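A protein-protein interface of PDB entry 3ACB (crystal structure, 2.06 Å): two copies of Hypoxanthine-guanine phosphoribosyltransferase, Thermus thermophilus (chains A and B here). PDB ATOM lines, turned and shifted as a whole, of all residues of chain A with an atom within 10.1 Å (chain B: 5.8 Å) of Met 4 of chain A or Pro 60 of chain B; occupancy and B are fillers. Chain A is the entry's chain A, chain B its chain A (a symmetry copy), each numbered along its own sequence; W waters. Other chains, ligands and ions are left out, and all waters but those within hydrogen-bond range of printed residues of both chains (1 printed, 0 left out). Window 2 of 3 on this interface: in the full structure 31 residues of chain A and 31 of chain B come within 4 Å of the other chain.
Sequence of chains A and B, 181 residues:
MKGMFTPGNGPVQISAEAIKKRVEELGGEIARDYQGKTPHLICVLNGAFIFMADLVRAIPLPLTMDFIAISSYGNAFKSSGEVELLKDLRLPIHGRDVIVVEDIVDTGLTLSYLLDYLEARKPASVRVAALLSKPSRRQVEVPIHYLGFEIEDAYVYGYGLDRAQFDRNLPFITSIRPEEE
Water W1 bridges the backbone carbonyl oxygen of Pro 171 of chain A (2.7 Å) and the guanidinium group of Arg 57 of chain B (3.0 Å).
Printed residues of chain A that touch a printed residue of chain B: Gly 3, Met 4, Phe 5 and Asn 169. Among the printed residues, 9 pairs touch across the chains.
Among the printed residues, pairs that only touch across the chains: Gly 3 of chain A with Pro 60 of chain B (3.9 Å), Met 4 of chain A with Pro 60 of chain B (3.5 Å), Phe 5 of chain A with Arg 57 of chain B (3.3 Å), Phe 5 of chain A with Ile 59 of chain B (3.6 Å), Phe 5 of chain A with Pro 60 of chain B (3.8 Å), Asn 169 of chain A with Val 56 of chain B (3.2 Å) and Asn 169 of chain A with Arg 57 of chain B (3.5 Å).
The side-chain amide nitrogen of Asn 169 of chain A sits at hydrogen-bond distance from the backbone carbonyl oxygen of Ile 59 of chain B (3.0 Å). The side-chain amide nitrogen (ND2) of Asn 169 of chain A sits at hydrogen-bond distance from the backbone carbonyl oxygen (O) of Leu 61 of chain B (3.0 Å).
The backbone carbonyl oxygen of Met 4 of chain A is in hydrogen-bond range of the side-chain hydroxyl of Thr 6 of chain A, at 3.2 Å.
No position is printed for both chains. Of the 9 pairs that touch across the chains among the printed residues, none has its exchanged pair printed and touching as well.
Pro 60 of chain B touches three residues of chain A. No residue of chain A comes within 4 Å of Ala 58 of chain B. Of the printed residues of chain B, Asn 169 of chain A touches Val 56 (3.2 Å), Arg 57 (3.5 Å), Ile 59 (3.0 Å) and Leu 61 (3.0 Å). Of the printed residues of chain A, Arg 57 of chain B touches Phe 5 (3.3 Å) and Asn 169 (3.5 Å). Of the printed residues of chain B, Gly 3 of chain A touches Pro 60 (3.9 Å). Printed residues of chain A within 4 Å of Ile 59 of chain B: Phe 5 and Asn 169. The nearest residue of chain B that does not touch Met 4 of chain A is Leu 61 of chain B (5.4 Å). The nearest residue of chain A that does not touch Pro 60 of chain B is Asn 169 of chain A (5.0 Å). The nearest printed residue of chain A that does not touch Val 56 of chain B is Phe 5 of chain A (4.2 Å).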
ATOM      1  N   GLY A   3       3.706   1.113  30.103  1.00  0.00           N
ATOM      2  CA  GLY A   3       2.390   0.787  30.723  1.00  0.00           C
ATOM      3  C   GLY A   3       1.955   1.821  31.743  1.00  0.00           C
ATOM      4  O   GLY A   3       2.776   2.336  32.501  1.00  0.00           O
ATOM      5  N   MET A   4       0.659   2.122  31.761  1.00  0.00           N
ATOM      6  CA  MET A   4       0.088   3.101  32.685  1.00  0.00           C
ATOM      7  C   MET A   4      -1.431   2.964  32.781  1.00  0.00           C
ATOM      8  O   MET A   4      -2.077   3.717  33.508  1.00  0.00           O
ATOM      9  CB  MET A   4       0.423   4.529  32.234  1.00  0.00           C
ATOM     10  CG  MET A   4       1.874   4.941  32.409  1.00  0.00           C
ATOM     11  SD  MET A   4       2.398   4.933  34.136  1.00  0.00           S
ATOM     12  CE  MET A   4       2.044   6.627  34.609  1.00  0.00           C
ATOM     13  N   PHE A   5      -2.004   2.013  32.047  1.00  0.00           N
ATOM     14  CA  PHE A   5      -3.455   1.822  32.072  1.00  0.00           C
ATOM     15  C   PHE A   5      -3.929   1.388  33.455  1.00  0.00           C
ATOM     16  O   PHE A   5      -3.557   0.320  33.949  1.00  0.00           O
ATOM     17  CB  PHE A   5      -3.880   0.788  31.023  1.00  0.00           C
ATOM     18  CG  PHE A   5      -3.646   1.230  29.602  1.00  0.00           C
ATOM     19  CD1 PHE A   5      -4.136   2.455  29.151  1.00  0.00           C
ATOM     20  CD2 PHE A   5      -2.940   0.422  28.717  1.00  0.00           C
ATOM     21  CE1 PHE A   5      -3.928   2.870  27.832  1.00  0.00           C
ATOM     22  CE2 PHE A   5      -2.724   0.822  27.395  1.00  0.00           C
ATOM     23  CZ  PHE A   5      -3.219   2.051  26.952  1.00  0.00           C
ATOM     24  N   THR A   6      -4.764   2.217  34.070  1.00  0.00           N
ATOM     25  CA  THR A   6      -5.273   1.936  35.405  1.00  0.00           C
ATOM     26  C   THR A   6      -6.798   1.926  35.478  1.00  0.00           C
ATOM     27  O   THR A   6      -7.457   2.868  35.041  1.00  0.00           O
ATOM     28  CB  THR A   6      -4.744   2.977  36.408  1.00  0.00           C
ATOM     29  OG1 THR A   6      -3.311   2.967  36.391  1.00  0.00           O
ATOM     30  CG2 THR A   6      -5.232   2.665  37.814  1.00  0.00           C
ATOM     31  N   PRO A   7      -7.377   0.855  36.040  1.00  0.00           N
ATOM     32  CA  PRO A   7      -8.834   0.752  36.161  1.00  0.00           C
ATOM     33  C   PRO A   7      -9.389   1.670  37.247  1.00  0.00           C
ATOM     34  O   PRO A   7      -8.679   2.039  38.189  1.00  0.00           O
ATOM     35  CB  PRO A   7      -9.047  -0.722  36.488  1.00  0.00           C
ATOM     36  CG  PRO A   7      -7.832  -1.052  37.300  1.00  0.00           C
ATOM     37  CD  PRO A   7      -6.723  -0.378  36.518  1.00  0.00           C
ATOM     38  N   GLY A   8     -10.655   2.040  37.105  1.00  0.00           N
ATOM     39  CA  GLY A   8     -11.288   2.895  38.089  1.00  0.00           C
ATOM     40  C   GLY A   8     -11.679   2.051  39.287  1.00  0.00           C
ATOM     41  O   GLY A   8     -11.448   0.840  39.293  1.00  0.00           O
ATOM     42  N   TYR A 157     -16.427   3.154  31.248  1.00  0.00           N
ATOM     43  CA  TYR A 157     -15.600   3.768  30.223  1.00  0.00           C
ATOM     44  C   TYR A 157     -14.462   2.841  29.824  1.00  0.00           C
ATOM     45  O   TYR A 157     -14.245   1.796  30.451  1.00  0.00           O
ATOM     46  CB  TYR A 157     -15.059   5.119  30.712  1.00  0.00           C
ATOM     47  CG  TYR A 157     -14.205   5.057  31.962  1.00  0.00           C
ATOM     48  CD1 TYR A 157     -12.813   5.049  31.876  1.00  0.00           C
ATOM     49  CD2 TYR A 157     -14.789   5.022  33.233  1.00  0.00           C
ATOM     50  CE1 TYR A 157     -12.019   5.013  33.022  1.00  0.00           C
ATOM     51  CE2 TYR A 157     -14.003   4.983  34.388  1.00  0.00           C
ATOM     52  CZ  TYR A 157     -12.618   4.980  34.272  1.00  0.00           C
ATOM     53  OH  TYR A 157     -11.829   4.949  35.400  1.00  0.00           O
ATOM     54  N   ARG A 163     -14.573   9.085  29.104  1.00  0.00           N
ATOM     55  CA  ARG A 163     -14.812   9.669  30.414  1.00  0.00           C
ATOM     56  C   ARG A 163     -14.406  11.118  30.143  1.00  0.00           C
ATOM     57  O   ARG A 163     -13.230  11.472  30.239  1.00  0.00           O
ATOM     58  CB  ARG A 163     -13.903   9.029  31.470  1.00  0.00           C
ATOM     59  CG  ARG A 163     -14.139   9.530  32.890  1.00  0.00           C
ATOM     60  CD  ARG A 163     -13.274   8.773  33.898  1.00  0.00           C
ATOM     61  NE  ARG A 163     -11.846   8.903  33.613  1.00  0.00           N
ATOM     62  CZ  ARG A 163     -11.157  10.040  33.710  1.00  0.00           C
ATOM     63  NH1 ARG A 163     -11.763  11.159  34.091  1.00  0.00           N
ATOM     64  NH2 ARG A 163      -9.859  10.062  33.417  1.00  0.00           N
ATOM     65  N   ASP A 167      -9.720   8.528  28.119  1.00  0.00           N
ATOM     66  CA  ASP A 167      -9.766   7.094  28.375  1.00  0.00           C
ATOM     67  C   ASP A 167     -10.394   6.139  27.369  1.00  0.00           C
ATOM     68  O   ASP A 167     -10.626   4.974  27.706  1.00  0.00           O
ATOM     69  CB  ASP A 167     -10.399   6.839  29.745  1.00  0.00           C
ATOM     70  CG  ASP A 167      -9.610   7.475  30.877  1.00  0.00           C
ATOM     71  OD1 ASP A 167      -8.363   7.412  30.848  1.00  0.00           O
ATOM     72  OD2 ASP A 167     -10.239   8.028  31.800  1.00  0.00           O
ATOM     73  N   ASN A 169      -8.918   4.999  25.063  1.00  0.00           N
ATOM     74  CA  ASN A 169      -7.807   4.115  24.719  1.00  0.00           C
ATOM     75  C   ASN A 169      -7.518   2.970  25.689  1.00  0.00           C
ATOM     76  O   ASN A 169      -6.641   2.141  25.436  1.00  0.00           O
ATOM     77  CB  ASN A 169      -6.537   4.941  24.467  1.00  0.00           C
ATOM     78  CG  ASN A 169      -6.137   5.793  25.654  1.00  0.00           C
ATOM     79  OD1 ASN A 169      -6.982   6.387  26.325  1.00  0.00           O
ATOM     80  ND2 ASN A 169      -4.840   5.880  25.901  1.00  0.00           N
ATOM     81  N   LEU A 170      -8.252   2.911  26.793  1.00  0.00           N
ATOM     82  CA  LEU A 170      -8.062   1.818  27.741  1.00  0.00           C
ATOM     83  C   LEU A 170      -8.431   0.525  27.018  1.00  0.00           C
ATOM     84  O   LEU A 170      -9.471   0.446  26.372  1.00  0.00           O
ATOM     85  CB  LEU A 170      -8.962   2.006  28.967  1.00  0.00           C
ATOM     86  CG  LEU A 170      -8.427   2.863  30.120  1.00  0.00           C
ATOM     87  CD1 LEU A 170      -7.884   4.187  29.613  1.00  0.00           C
ATOM     88  CD2 LEU A 170      -9.544   3.086  31.121  1.00  0.00           C
ATOM     89  N   PRO A 171      -7.572  -0.503  27.103  1.00  0.00           N
ATOM     90  CA  PRO A 171      -7.864  -1.774  26.431  1.00  0.00           C
ATOM     91  C   PRO A 171      -8.918  -2.615  27.145  1.00  0.00           C
ATOM     92  O   PRO A 171      -9.326  -3.665  26.652  1.00  0.00           O
ATOM     93  CB  PRO A 171      -6.499  -2.458  26.379  1.00  0.00           C
ATOM     94  CG  PRO A 171      -5.829  -1.955  27.618  1.00  0.00           C
ATOM     95  CD  PRO A 171      -6.199  -0.490  27.642  1.00  0.00           C
ATOM     96  N   PHE A 172      -9.364  -2.142  28.300  1.00  0.00           N
ATOM     97  CA  PHE A 172     -10.366  -2.864  29.073  1.00  0.00           C
ATOM     98  C   PHE A 172     -11.516  -1.941  29.424  1.00  0.00           C
ATOM     99  O   PHE A 172     -11.424  -0.731  29.221  1.00  0.00           O
ATOM    100  CB  PHE A 172      -9.732  -3.414  30.357  1.00  0.00           C
ATOM    101  CG  PHE A 172      -8.979  -2.380  31.153  1.00  0.00           C
ATOM    102  CD1 PHE A 172      -9.658  -1.405  31.878  1.00  0.00           C
ATOM    103  CD2 PHE A 172      -7.586  -2.366  31.155  1.00  0.00           C
ATOM    104  CE1 PHE A 172      -8.963  -0.428  32.590  1.00  0.00           C
ATOM    105  CE2 PHE A 172      -6.878  -1.395  31.861  1.00  0.00           C
ATOM    106  CZ  PHE A 172      -7.569  -0.421  32.581  1.00  0.00           C
ATOM    107  N   GLY B  27       3.059   2.713  18.991  1.00  0.00           N
ATOM    108  CA  GLY B  27       2.395   3.201  20.188  1.00  0.00           C
ATOM    109  C   GLY B  27       3.422   3.538  21.257  1.00  0.00           C
ATOM    110  O   GLY B  27       3.303   4.543  21.967  1.00  0.00           O
ATOM    111  N   ALA B  31       4.044   7.180  22.996  1.00  0.00           N
ATOM    112  CA  ALA B  31       3.980   7.312  24.452  1.00  0.00           C
ATOM    113  C   ALA B  31       5.254   7.973  24.971  1.00  0.00           C
ATOM    114  O   ALA B  31       5.206   8.831  25.850  1.00  0.00           O
ATOM    115  CB  ALA B  31       3.802   5.941  25.104  1.00  0.00           C
ATOM    116  N   VAL B  56      -4.261   3.248  19.550  1.00  0.00           N
ATOM    117  CA  VAL B  56      -4.585   3.939  20.796  1.00  0.00           C
ATOM    118  C   VAL B  56      -4.418   3.033  22.011  1.00  0.00           C
ATOM    119  O   VAL B  56      -3.993   3.477  23.080  1.00  0.00           O
ATOM    120  CB  VAL B  56      -6.014   4.515  20.778  1.00  0.00           C
ATOM    121  CG1 VAL B  56      -6.140   5.542  19.657  1.00  0.00           C
ATOM    122  CG2 VAL B  56      -7.033   3.398  20.617  1.00  0.00           C
ATOM    123  N   ARG B  57      -4.734   1.757  21.844  1.00  0.00           N
ATOM    124  CA  ARG B  57      -4.594   0.814  22.937  1.00  0.00           C
ATOM    125  C   ARG B  57      -3.129   0.514  23.242  1.00  0.00           C
ATOM    126  O   ARG B  57      -2.824  -0.177  24.214  1.00  0.00           O
ATOM    127  CB  ARG B  57      -5.353  -0.470  22.616  1.00  0.00           C
ATOM    128  CG  ARG B  57      -6.856  -0.300  22.767  1.00  0.00           C
ATOM    129  CD  ARG B  57      -7.605  -1.567  22.441  1.00  0.00           C
ATOM    130  NE  ARG B  57      -7.633  -1.820  21.006  1.00  0.00           N
ATOM    131  CZ  ARG B  57      -8.226  -2.871  20.456  1.00  0.00           C
ATOM    132  NH1 ARG B  57      -8.835  -3.764  21.226  1.00  0.00           N
ATOM    133  NH2 ARG B  57      -8.223  -3.019  19.141  1.00  0.00           N
ATOM    134  N   ALA B  58      -2.228   1.047  22.417  1.00  0.00           N
ATOM    135  CA  ALA B  58      -0.795   0.850  22.612  1.00  0.00           C
ATOM    136  C   ALA B  58      -0.118   2.139  23.080  1.00  0.00           C
ATOM    137  O   ALA B  58       1.112   2.234  23.086  1.00  0.00           O
ATOM    138  CB  ALA B  58      -0.147   0.365  21.318  1.00  0.00           C
ATOM    139  N   ILE B  59      -0.921   3.131  23.458  1.00  0.00           N
ATOM    140  CA  ILE B  59      -0.383   4.402  23.935  1.00  0.00           C
ATOM    141  C   ILE B  59      -0.870   4.661  25.357  1.00  0.00           C
ATOM    142  O   ILE B  59      -1.971   5.185  25.564  1.00  0.00           O
ATOM    143  CB  ILE B  59      -0.827   5.585  23.044  1.00  0.00           C
ATOM    144  CG1 ILE B  59      -0.398   5.344  21.595  1.00  0.00           C
ATOM    145  CG2 ILE B  59      -0.209   6.883  23.564  1.00  0.00           C
ATOM    146  CD1 ILE B  59      -0.893   6.403  20.627  1.00  0.00           C
ATOM    147  N   PRO B  60      -0.055   4.292  26.359  1.00  0.00           N
ATOM    148  CA  PRO B  60      -0.389   4.475  27.777  1.00  0.00           C
ATOM    149  C   PRO B  60      -0.333   5.930  28.237  1.00  0.00           C
ATOM    150  O   PRO B  60       0.423   6.267  29.146  1.00  0.00           O
ATOM    151  CB  PRO B  60       0.653   3.611  28.496  1.00  0.00           C
ATOM    152  CG  PRO B  60       1.052   2.597  27.461  1.00  0.00           C
ATOM    153  CD  PRO B  60       1.132   3.432  26.214  1.00  0.00           C
ATOM    154  N   LEU B  61      -1.130   6.788  27.613  1.00  0.00           N
ATOM    155  CA  LEU B  61      -1.162   8.201  27.986  1.00  0.00           C
ATOM    156  C   LEU B  61      -2.588   8.729  27.984  1.00  0.00           C
ATOM    157  O   LEU B  61      -3.460   8.183  27.308  1.00  0.00           O
ATOM    158  CB  LEU B  61      -0.358   9.048  26.992  1.00  0.00           C
ATOM    159  CG  LEU B  61       1.163   8.936  26.874  1.00  0.00           C
ATOM    160  CD1 LEU B  61       1.632   9.801  25.711  1.00  0.00           C
ATOM    161  CD2 LEU B  61       1.825   9.383  28.169  1.00  0.00           C
ATOM    162  N   PRO B  62      -2.849   9.789  28.760  1.00  0.00           N
ATOM    163  CA  PRO B  62      -4.213  10.317  28.746  1.00  0.00           C
ATOM    164  C   PRO B  62      -4.318  11.029  27.402  1.00  0.00           C
ATOM    165  O   PRO B  62      -3.442  11.817  27.042  1.00  0.00           O
ATOM    166  CB  PRO B  62      -4.227  11.283  29.927  1.00  0.00           C
ATOM    167  CG  PRO B  62      -2.791  11.744  30.009  1.00  0.00           C
ATOM    168  CD  PRO B  62      -2.024  10.464  29.778  1.00  0.00           C
HETATM  169  O   HOH W   1      -8.640  -4.356  24.111  1.00  0.00           O
